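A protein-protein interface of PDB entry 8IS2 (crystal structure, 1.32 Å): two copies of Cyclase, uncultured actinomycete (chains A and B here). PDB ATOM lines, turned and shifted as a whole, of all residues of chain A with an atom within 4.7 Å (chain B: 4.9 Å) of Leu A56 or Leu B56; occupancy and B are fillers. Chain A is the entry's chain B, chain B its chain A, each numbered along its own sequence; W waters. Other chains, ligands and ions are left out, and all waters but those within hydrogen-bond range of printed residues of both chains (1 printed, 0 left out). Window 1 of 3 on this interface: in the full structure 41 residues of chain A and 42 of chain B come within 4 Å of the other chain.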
ATOM      1  N   THR A   7      31.515 -26.174  30.485  1.00  0.00           N
ATOM      2  CA  THR A   7      30.415 -25.574  29.748  1.00  0.00           C
ATOM      3  C   THR A   7      30.246 -26.319  28.435  1.00  0.00           C
ATOM      4  O   THR A   7      31.215 -26.505  27.694  1.00  0.00           O
ATOM      5  CB  THR A   7      30.678 -24.085  29.512  1.00  0.00           C
ATOM      6  OG1 THR A   7      30.649 -23.393  30.770  1.00  0.00           O
ATOM      7  CG2 THR A   7      29.627 -23.498  28.600  1.00  0.00           C
ATOM      8  N   THR A   8      29.030 -26.763  28.159  1.00  0.00           N
ATOM      9  CA  THR A   8      28.722 -27.531  26.962  1.00  0.00           C
ATOM     10  C   THR A   8      27.608 -26.835  26.195  1.00  0.00           C
ATOM     11  O   THR A   8      26.613 -26.395  26.778  1.00  0.00           O
ATOM     12  CB  THR A   8      28.262 -28.946  27.348  1.00  0.00           C
ATOM     13  OG1 THR A   8      29.286 -29.597  28.102  1.00  0.00           O
ATOM     14  CG2 THR A   8      27.967 -29.789  26.127  1.00  0.00           C
ATOM     15  N   LEU A   9      27.776 -26.745  24.879  1.00  0.00           N
ATOM     16  CA  LEU A   9      26.772 -26.169  23.996  1.00  0.00           C
ATOM     17  C   LEU A   9      26.364 -27.211  22.965  1.00  0.00           C
ATOM     18  O   LEU A   9      27.188 -27.635  22.146  1.00  0.00           O
ATOM     19  CB  LEU A   9      27.340 -24.942  23.292  1.00  0.00           C
ATOM     20  CG  LEU A   9      26.491 -24.275  22.213  1.00  0.00           C
ATOM     21  CD1 LEU A   9      25.200 -23.718  22.771  1.00  0.00           C
ATOM     22  CD2 LEU A   9      27.297 -23.159  21.587  1.00  0.00           C
ATOM     23  N   GLU A  43      24.004 -24.356  35.915  1.00  0.00           N
ATOM     24  CA  GLU A  43      23.176 -23.414  35.173  1.00  0.00           C
ATOM     25  C   GLU A  43      22.842 -24.016  33.815  1.00  0.00           C
ATOM     26  O   GLU A  43      23.675 -24.700  33.213  1.00  0.00           O
ATOM     27  CB  GLU A  43      23.940 -22.092  34.999  1.00  0.00           C
ATOM     28  CG  GLU A  43      23.097 -20.893  34.606  1.00  0.00           C
ATOM     29  CD  GLU A  43      23.880 -19.584  34.685  1.00  0.00           C
ATOM     30  OE1 GLU A  43      25.105 -19.623  34.932  1.00  0.00           O
ATOM     31  OE2 GLU A  43      23.268 -18.513  34.504  1.00  0.00           O
ATOM     32  N   ARG A  44      21.630 -23.749  33.338  1.00  0.00           N
ATOM     33  CA  ARG A  44      21.152 -24.236  32.047  1.00  0.00           C
ATOM     34  C   ARG A  44      20.463 -23.082  31.337  1.00  0.00           C
ATOM     35  O   ARG A  44      19.666 -22.368  31.955  1.00  0.00           O
ATOM     36  CB  ARG A  44      20.167 -25.416  32.182  1.00  0.00           C
ATOM     37  CG  ARG A  44      19.816 -26.106  30.860  1.00  0.00           C
ATOM     38  CD  ARG A  44      18.601 -27.051  30.965  1.00  0.00           C
ATOM     39  NE  ARG A  44      18.661 -27.905  32.139  1.00  0.00           N
ATOM     40  CZ  ARG A  44      19.429 -28.981  32.247  1.00  0.00           C
ATOM     41  NH1 ARG A  44      20.235 -29.356  31.267  1.00  0.00           N
ATOM     42  NH2 ARG A  44      19.405 -29.686  33.376  1.00  0.00           N
ATOM     43  N   ARG A  45      20.784 -22.891  30.056  1.00  0.00           N
ATOM     44  CA  ARG A  45      20.134 -21.901  29.209  1.00  0.00           C
ATOM     45  C   ARG A  45      19.727 -22.566  27.902  1.00  0.00           C
ATOM     46  O   ARG A  45      20.538 -23.262  27.277  1.00  0.00           O
ATOM     47  CB  ARG A  45      21.074 -20.731  28.920  1.00  0.00           C
ATOM     48  CG  ARG A  45      21.399 -19.884  30.135  1.00  0.00           C
ATOM     49  CD  ARG A  45      22.498 -18.912  29.815  1.00  0.00           C
ATOM     50  NE  ARG A  45      23.023 -18.272  31.013  1.00  0.00           N
ATOM     51  CZ  ARG A  45      22.604 -17.105  31.480  1.00  0.00           C
ATOM     52  NH1 ARG A  45      21.654 -16.419  30.863  1.00  0.00           N
ATOM     53  NH2 ARG A  45      23.178 -16.595  32.567  1.00  0.00           N
ATOM     54  N   LEU A  47      18.172 -21.609  24.082  1.00  0.00           N
ATOM     55  CA  LEU A  47      18.055 -20.465  23.193  1.00  0.00           C
ATOM     56  C   LEU A  47      17.682 -20.937  21.793  1.00  0.00           C
ATOM     57  O   LEU A  47      17.857 -22.110  21.440  1.00  0.00           O
ATOM     58  CB  LEU A  47      19.372 -19.680  23.134  1.00  0.00           C
ATOM     59  CG  LEU A  47      20.089 -19.423  24.458  1.00  0.00           C
ATOM     60  CD1 LEU A  47      21.032 -20.558  24.789  1.00  0.00           C
ATOM     61  CD2 LEU A  47      20.830 -18.092  24.479  1.00  0.00           C
ATOM     62  N   PHE A  54      19.707 -24.271  20.744  1.00  0.00           N
ATOM     63  CA  PHE A  54      20.934 -24.340  21.520  1.00  0.00           C
ATOM     64  C   PHE A  54      20.596 -24.680  22.956  1.00  0.00           C
ATOM     65  O   PHE A  54      19.716 -24.055  23.561  1.00  0.00           O
ATOM     66  CB  PHE A  54      21.694 -23.018  21.500  1.00  0.00           C
ATOM     67  CG  PHE A  54      21.946 -22.484  20.117  1.00  0.00           C
ATOM     68  CD1 PHE A  54      22.669 -23.215  19.180  1.00  0.00           C
ATOM     69  CD2 PHE A  54      21.454 -21.239  19.747  1.00  0.00           C
ATOM     70  CE1 PHE A  54      22.886 -22.711  17.902  1.00  0.00           C
ATOM     71  CE2 PHE A  54      21.673 -20.731  18.489  1.00  0.00           C
ATOM     72  CZ  PHE A  54      22.393 -21.464  17.561  1.00  0.00           C
ATOM     73  N   HIS A  55      21.287 -25.670  23.500  1.00  0.00           N
ATOM     74  CA  HIS A  55      21.165 -26.060  24.898  1.00  0.00           C
ATOM     75  C   HIS A  55      22.542 -25.810  25.495  1.00  0.00           C
ATOM     76  O   HIS A  55      23.517 -26.460  25.104  1.00  0.00           O
ATOM     77  CB  HIS A  55      20.755 -27.530  24.999  1.00  0.00           C
ATOM     78  CG  HIS A  55      20.681 -28.063  26.399  1.00  0.00           C
ATOM     79  ND1 HIS A  55      20.292 -29.357  26.673  1.00  0.00           N
ATOM     80  CD2 HIS A  55      20.931 -27.486  27.599  1.00  0.00           C
ATOM     81  CE1 HIS A  55      20.311 -29.556  27.978  1.00  0.00           C
ATOM     82  NE2 HIS A  55      20.695 -28.435  28.564  1.00  0.00           N
ATOM     83  N   LEU A  56      22.623 -24.851  26.409  1.00  0.00           N
ATOM     84  CA  LEU A  56      23.866 -24.442  27.039  1.00  0.00           C
ATOM     85  C   LEU A  56      23.805 -24.826  28.518  1.00  0.00           C
ATOM     86  O   LEU A  56      22.899 -24.395  29.256  1.00  0.00           O
ATOM     87  CB  LEU A  56      24.049 -22.938  26.864  1.00  0.00           C
ATOM     88  CG  LEU A  56      25.274 -22.249  27.447  1.00  0.00           C
ATOM     89  CD1 LEU A  56      26.540 -22.740  26.771  1.00  0.00           C
ATOM     90  CD2 LEU A  56      25.123 -20.743  27.307  1.00  0.00           C
ATOM     91  N   VAL A  57      24.758 -25.650  28.953  1.00  0.00           N
ATOM     92  CA  VAL A  57      24.779 -26.172  30.316  1.00  0.00           C
ATOM     93  C   VAL A  57      26.163 -25.990  30.919  1.00  0.00           C
ATOM     94  O   VAL A  57      27.179 -26.253  30.269  1.00  0.00           O
ATOM     95  CB  VAL A  57      24.313 -27.646  30.384  1.00  0.00           C
ATOM     96  CG1 VAL A  57      25.279 -28.564  29.674  1.00  0.00           C
ATOM     97  CG2 VAL A  57      24.113 -28.082  31.824  1.00  0.00           C
ATOM     98  N   ARG A  58      26.202 -25.503  32.154  1.00  0.00           N
ATOM     99  CA  ARG A  58      27.422 -25.409  32.943  1.00  0.00           C
ATOM    100  C   ARG A  58      27.306 -26.414  34.078  1.00  0.00           C
ATOM    101  O   ARG A  58      26.287 -26.447  34.772  1.00  0.00           O
ATOM    102  CB  ARG A  58      27.573 -23.996  33.510  1.00  0.00           C
ATOM    103  CG  ARG A  58      28.834 -23.766  34.328  1.00  0.00           C
ATOM    104  CD  ARG A  58      28.763 -22.451  35.111  1.00  0.00           C
ATOM    105  NE  ARG A  58      29.259 -21.304  34.356  1.00  0.00           N
ATOM    106  CZ  ARG A  58      28.502 -20.492  33.626  1.00  0.00           C
ATOM    107  NH1 ARG A  58      27.200 -20.685  33.500  1.00  0.00           N
ATOM    108  NH2 ARG A  58      29.066 -19.456  33.012  1.00  0.00           N
ATOM    109  N   THR B   7      24.452 -12.670  29.847  1.00  0.00           N
ATOM    110  CA  THR B   7      25.162 -13.613  28.994  1.00  0.00           C
ATOM    111  C   THR B   7      24.526 -13.578  27.611  1.00  0.00           C
ATOM    112  O   THR B   7      23.296 -13.647  27.480  1.00  0.00           O
ATOM    113  CB  THR B   7      25.112 -15.022  29.603  1.00  0.00           C
ATOM    114  OG1 THR B   7      25.899 -15.042  30.800  1.00  0.00           O
ATOM    115  CG2 THR B   7      25.675 -16.055  28.656  1.00  0.00           C
ATOM    116  N   THR B   8      25.356 -13.421  26.588  1.00  0.00           N
ATOM    117  CA  THR B   8      24.903 -13.333  25.206  1.00  0.00           C
ATOM    118  C   THR B   8      25.601 -14.405  24.389  1.00  0.00           C
ATOM    119  O   THR B   8      26.805 -14.610  24.537  1.00  0.00           O
ATOM    120  CB  THR B   8      25.248 -11.961  24.606  1.00  0.00           C
ATOM    121  OG1 THR B   8      24.737 -10.930  25.446  1.00  0.00           O
ATOM    122  CG2 THR B   8      24.632 -11.808  23.236  1.00  0.00           C
ATOM    123  N   LEU B   9      24.834 -15.094  23.536  1.00  0.00           N
ATOM    124  CA  LEU B   9      25.372 -16.063  22.579  1.00  0.00           C
ATOM    125  C   LEU B   9      25.209 -15.500  21.171  1.00  0.00           C
ATOM    126  O   LEU B   9      24.086 -15.355  20.678  1.00  0.00           O
ATOM    127  CB  LEU B   9      24.671 -17.416  22.685  1.00  0.00           C
ATOM    128  CG  LEU B   9      25.169 -18.489  21.714  1.00  0.00           C
ATOM    129  CD1 LEU B   9      26.607 -18.920  22.031  1.00  0.00           C
ATOM    130  CD2 LEU B   9      24.207 -19.687  21.671  1.00  0.00           C
ATOM    131  N   GLU B  43      33.766 -12.847  31.253  1.00  0.00           N
ATOM    132  CA  GLU B  43      34.216 -14.129  30.739  1.00  0.00           C
ATOM    133  C   GLU B  43      33.786 -14.236  29.288  1.00  0.00           C
ATOM    134  O   GLU B  43      32.710 -13.750  28.916  1.00  0.00           O
ATOM    135  CB  GLU B  43      33.598 -15.254  31.578  1.00  0.00           C
ATOM    136  CG  GLU B  43      34.194 -16.624  31.337  1.00  0.00           C
ATOM    137  CD  GLU B  43      33.828 -17.622  32.442  1.00  0.00           C
ATOM    138  OE1 GLU B  43      32.891 -17.354  33.223  1.00  0.00           O
ATOM    139  OE2 GLU B  43      34.481 -18.677  32.542  1.00  0.00           O
ATOM    140  N   ARG B  44      34.634 -14.847  28.473  1.00  0.00           N
ATOM    141  CA  ARG B  44      34.356 -14.992  27.055  1.00  0.00           C
ATOM    142  C   ARG B  44      34.774 -16.390  26.629  1.00  0.00           C
ATOM    143  O   ARG B  44      35.842 -16.867  27.023  1.00  0.00           O
ATOM    144  CB  ARG B  44      35.127 -13.982  26.208  1.00  0.00           C
ATOM    145  CG  ARG B  44      34.658 -13.909  24.767  1.00  0.00           C
ATOM    146  CD  ARG B  44      35.638 -13.206  23.861  1.00  0.00           C
ATOM    147  NE  ARG B  44      36.101 -11.936  24.407  1.00  0.00           N
ATOM    148  CZ  ARG B  44      35.374 -10.826  24.470  1.00  0.00           C
ATOM    149  NH1 ARG B  44      34.129 -10.784  24.023  1.00  0.00           N
ATOM    150  NH2 ARG B  44      35.908  -9.737  25.011  1.00  0.00           N
ATOM    151  N   ARG B  45      33.958 -17.021  25.785  1.00  0.00           N
ATOM    152  CA  ARG B  45      34.301 -18.288  25.166  1.00  0.00           C
ATOM    153  C   ARG B  45      33.934 -18.218  23.695  1.00  0.00           C
ATOM    154  O   ARG B  45      32.901 -17.638  23.348  1.00  0.00           O
ATOM    155  CB  ARG B  45      33.523 -19.443  25.819  1.00  0.00           C
ATOM    156  CG  ARG B  45      33.826 -19.661  27.296  1.00  0.00           C
ATOM    157  CD  ARG B  45      32.856 -20.672  27.897  1.00  0.00           C
ATOM    158  NE  ARG B  45      32.905 -20.708  29.357  1.00  0.00           N
ATOM    159  CZ  ARG B  45      33.519 -21.635  30.083  1.00  0.00           C
ATOM    160  NH1 ARG B  45      34.191 -22.627  29.520  1.00  0.00           N
ATOM    161  NH2 ARG B  45      33.445 -21.571  31.409  1.00  0.00           N
ATOM    162  N   LEU B  47      33.453 -20.886  20.313  1.00  0.00           N
ATOM    163  CA  LEU B  47      33.262 -22.286  19.990  1.00  0.00           C
ATOM    164  C   LEU B  47      32.933 -22.412  18.512  1.00  0.00           C
ATOM    165  O   LEU B  47      32.527 -21.449  17.854  1.00  0.00           O
ATOM    166  CB  LEU B  47      32.143 -22.927  20.821  1.00  0.00           C
ATOM    167  CG  LEU B  47      32.149 -22.637  22.327  1.00  0.00           C
ATOM    168  CD1 LEU B  47      31.393 -21.352  22.670  1.00  0.00           C
ATOM    169  CD2 LEU B  47      31.599 -23.832  23.135  1.00  0.00           C
ATOM    170  N   PHE B  54      30.463 -19.560  17.319  1.00  0.00           N
ATOM    171  CA  PHE B  54      29.752 -19.108  18.512  1.00  0.00           C
ATOM    172  C   PHE B  54      30.651 -18.231  19.361  1.00  0.00           C
ATOM    173  O   PHE B  54      31.794 -18.598  19.633  1.00  0.00           O
ATOM    174  CB  PHE B  54      29.255 -20.265  19.376  1.00  0.00           C
ATOM    175  CG  PHE B  54      28.323 -21.195  18.669  1.00  0.00           C
ATOM    176  CD1 PHE B  54      27.012 -20.828  18.472  1.00  0.00           C
ATOM    177  CD2 PHE B  54      28.756 -22.411  18.174  1.00  0.00           C
ATOM    178  CE1 PHE B  54      26.141 -21.667  17.814  1.00  0.00           C
ATOM    179  CE2 PHE B  54      27.891 -23.250  17.519  1.00  0.00           C
ATOM    180  CZ  PHE B  54      26.578 -22.875  17.333  1.00  0.00           C
ATOM    181  N   HIS B  55      30.129 -17.084  19.773  1.00  0.00           N
ATOM    182  CA  HIS B  55      30.804 -16.200  20.706  1.00  0.00           C
ATOM    183  C   HIS B  55      29.897 -16.077  21.924  1.00  0.00           C
ATOM    184  O   HIS B  55      28.802 -15.515  21.828  1.00  0.00           O
ATOM    185  CB  HIS B  55      31.064 -14.858  20.014  1.00  0.00           C
ATOM    186  CG  HIS B  55      31.577 -13.783  20.917  1.00  0.00           C
ATOM    187  ND1 HIS B  55      31.518 -12.453  20.567  1.00  0.00           N
ATOM    188  CD2 HIS B  55      32.153 -13.826  22.143  1.00  0.00           C
ATOM    189  CE1 HIS B  55      32.043 -11.722  21.534  1.00  0.00           C
ATOM    190  NE2 HIS B  55      32.426 -12.529  22.509  1.00  0.00           N
ATOM    191  N   LEU B  56      30.328 -16.635  23.048  1.00  0.00           N
ATOM    192  CA  LEU B  56      29.572 -16.629  24.291  1.00  0.00           C
ATOM    193  C   LEU B  56      30.274 -15.672  25.247  1.00  0.00           C
ATOM    194  O   LEU B  56      31.453 -15.871  25.561  1.00  0.00           O
ATOM    195  CB  LEU B  56      29.527 -18.029  24.881  1.00  0.00           C
ATOM    196  CG  LEU B  56      28.776 -18.171  26.189  1.00  0.00           C
ATOM    197  CD1 LEU B  56      27.295 -17.843  25.987  1.00  0.00           C
ATOM    198  CD2 LEU B  56      28.941 -19.566  26.723  1.00  0.00           C
ATOM    199  N   VAL B  57      29.570 -14.618  25.680  1.00  0.00           N
ATOM    200  CA  VAL B  57      30.193 -13.539  26.452  1.00  0.00           C
ATOM    201  C   VAL B  57      29.296 -13.128  27.617  1.00  0.00           C
ATOM    202  O   VAL B  57      28.090 -12.935  27.444  1.00  0.00           O
ATOM    203  CB  VAL B  57      30.591 -12.340  25.559  1.00  0.00           C
ATOM    204  CG1 VAL B  57      29.379 -11.702  24.906  1.00  0.00           C
ATOM    205  CG2 VAL B  57      31.397 -11.320  26.351  1.00  0.00           C
ATOM    206  N   ARG B  58      29.875 -13.036  28.808  1.00  0.00           N
ATOM    207  CA  ARG B  58      29.185 -12.601  30.016  1.00  0.00           C
ATOM    208  C   ARG B  58      29.721 -11.226  30.372  1.00  0.00           C
ATOM    209  O   ARG B  58      30.939 -11.052  30.501  1.00  0.00           O
ATOM    210  CB  ARG B  58      29.433 -13.586  31.160  1.00  0.00           C
ATOM    211  CG  ARG B  58      28.563 -13.335  32.363  1.00  0.00           C
ATOM    212  CD  ARG B  58      28.512 -14.566  33.242  1.00  0.00           C
ATOM    213  NE  ARG B  58      29.845 -15.044  33.592  1.00  0.00           N
ATOM    214  CZ  ARG B  58      30.578 -14.564  34.587  1.00  0.00           C
ATOM    215  NH1 ARG B  58      30.142 -13.577  35.355  1.00  0.00           N
ATOM    216  NH2 ARG B  58      31.778 -15.088  34.821  1.00  0.00           N
HETATM  217  O   HOH W   1      25.037 -13.799  33.170  1.00  0.00           O
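Water W1 bridges the side-chain hydroxyl (OG1) of Thr B7 (2.8 Å) and the guanidinium group (NH2) of Arg A45 (3.4 Å).
Thr A7 touches Arg B45, and with the chains exchanged Arg A45 touches Thr B7. Leu A9 touches Phe B54, and with the chains exchanged Phe A54 touches Leu B9. Phe A54 touches its own counterpart, Phe B54. Leu B56 touches its own counterpart, Leu A56. Positions printed for both chains: 7, 8, 9, 43, 44, 45, 47, 54, 55, 56, 57 and 58.
NH2 of Arg B45 sits at hydrogen-bond distance from OG1 of Thr A7.
Leu A56 touches just one residue of chain B: Leu B56 (3.9 Å). Of chain A, only Leu A56 comes within 4 Å of Leu B56. Of the printed residues of chain A, Arg B45 touches Thr A7. Of the printed residues of chain A, Leu B9 touches Phe A54. Printed residues of chain B within 4 Å of Arg A45: Thr B7. Of the printed residues of chain A, Thr B7 touches Arg A45. The nearest printed residue of chain B that does not touch Leu A56 is Thr B7 (4.9 Å).
Among the printed residues, pairs that only touch across the chains: Phe A54 with Phe B54, Arg A45 with Thr B7, Leu A9 with Phe B54, Phe A54 with Leu B9 and Leu A56 with Leu B56.
The backbone NH (N) of Phe B54 is in hydrogen-bond range of the backbone carbonyl oxygen (O) of Leu B47 (2.8 Å). The backbone carbonyl oxygen of Leu A56 lies within hydrogen-bond range of the backbone NH of Arg A45 (2.7 Å). The backbone NH (N) of Phe A54 sits at hydrogen-bond distance from the backbone carbonyl oxygen (O) of Leu A47, 2.9 Å away. OE2 of Glu B43 lies within salt-bridge range of NH2 of Arg B45 (3.3 Å). N of Arg B45 lies within hydrogen-bond range of O of Leu B56. The side-chain carboxylate of Glu A43 lies within salt-bridge range of the guanidinium group of Arg A45 (2.7 Å).
Printed residues of chain B that touch a printed residue of chain A: Thr B7, Leu B9, Arg B45, Phe B54 and Leu B56. Of the 12 printed residues of chain A, 5 touch a printed residue of chain B. Printed residues of chain A that touch a printed residue of chain B: Thr A7, Leu A9, Arg A45, Phe A54 and Leu A56. Along chain A the printed residues that touch a printed residue of chain B span positions 7 to 56. Among the printed residues, 6 pairs touch across the chains. Among the printed residues, no Asp or Glu carboxylate lies within 4 Å of a Lys or Arg side-chain nitrogen of the other chain.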
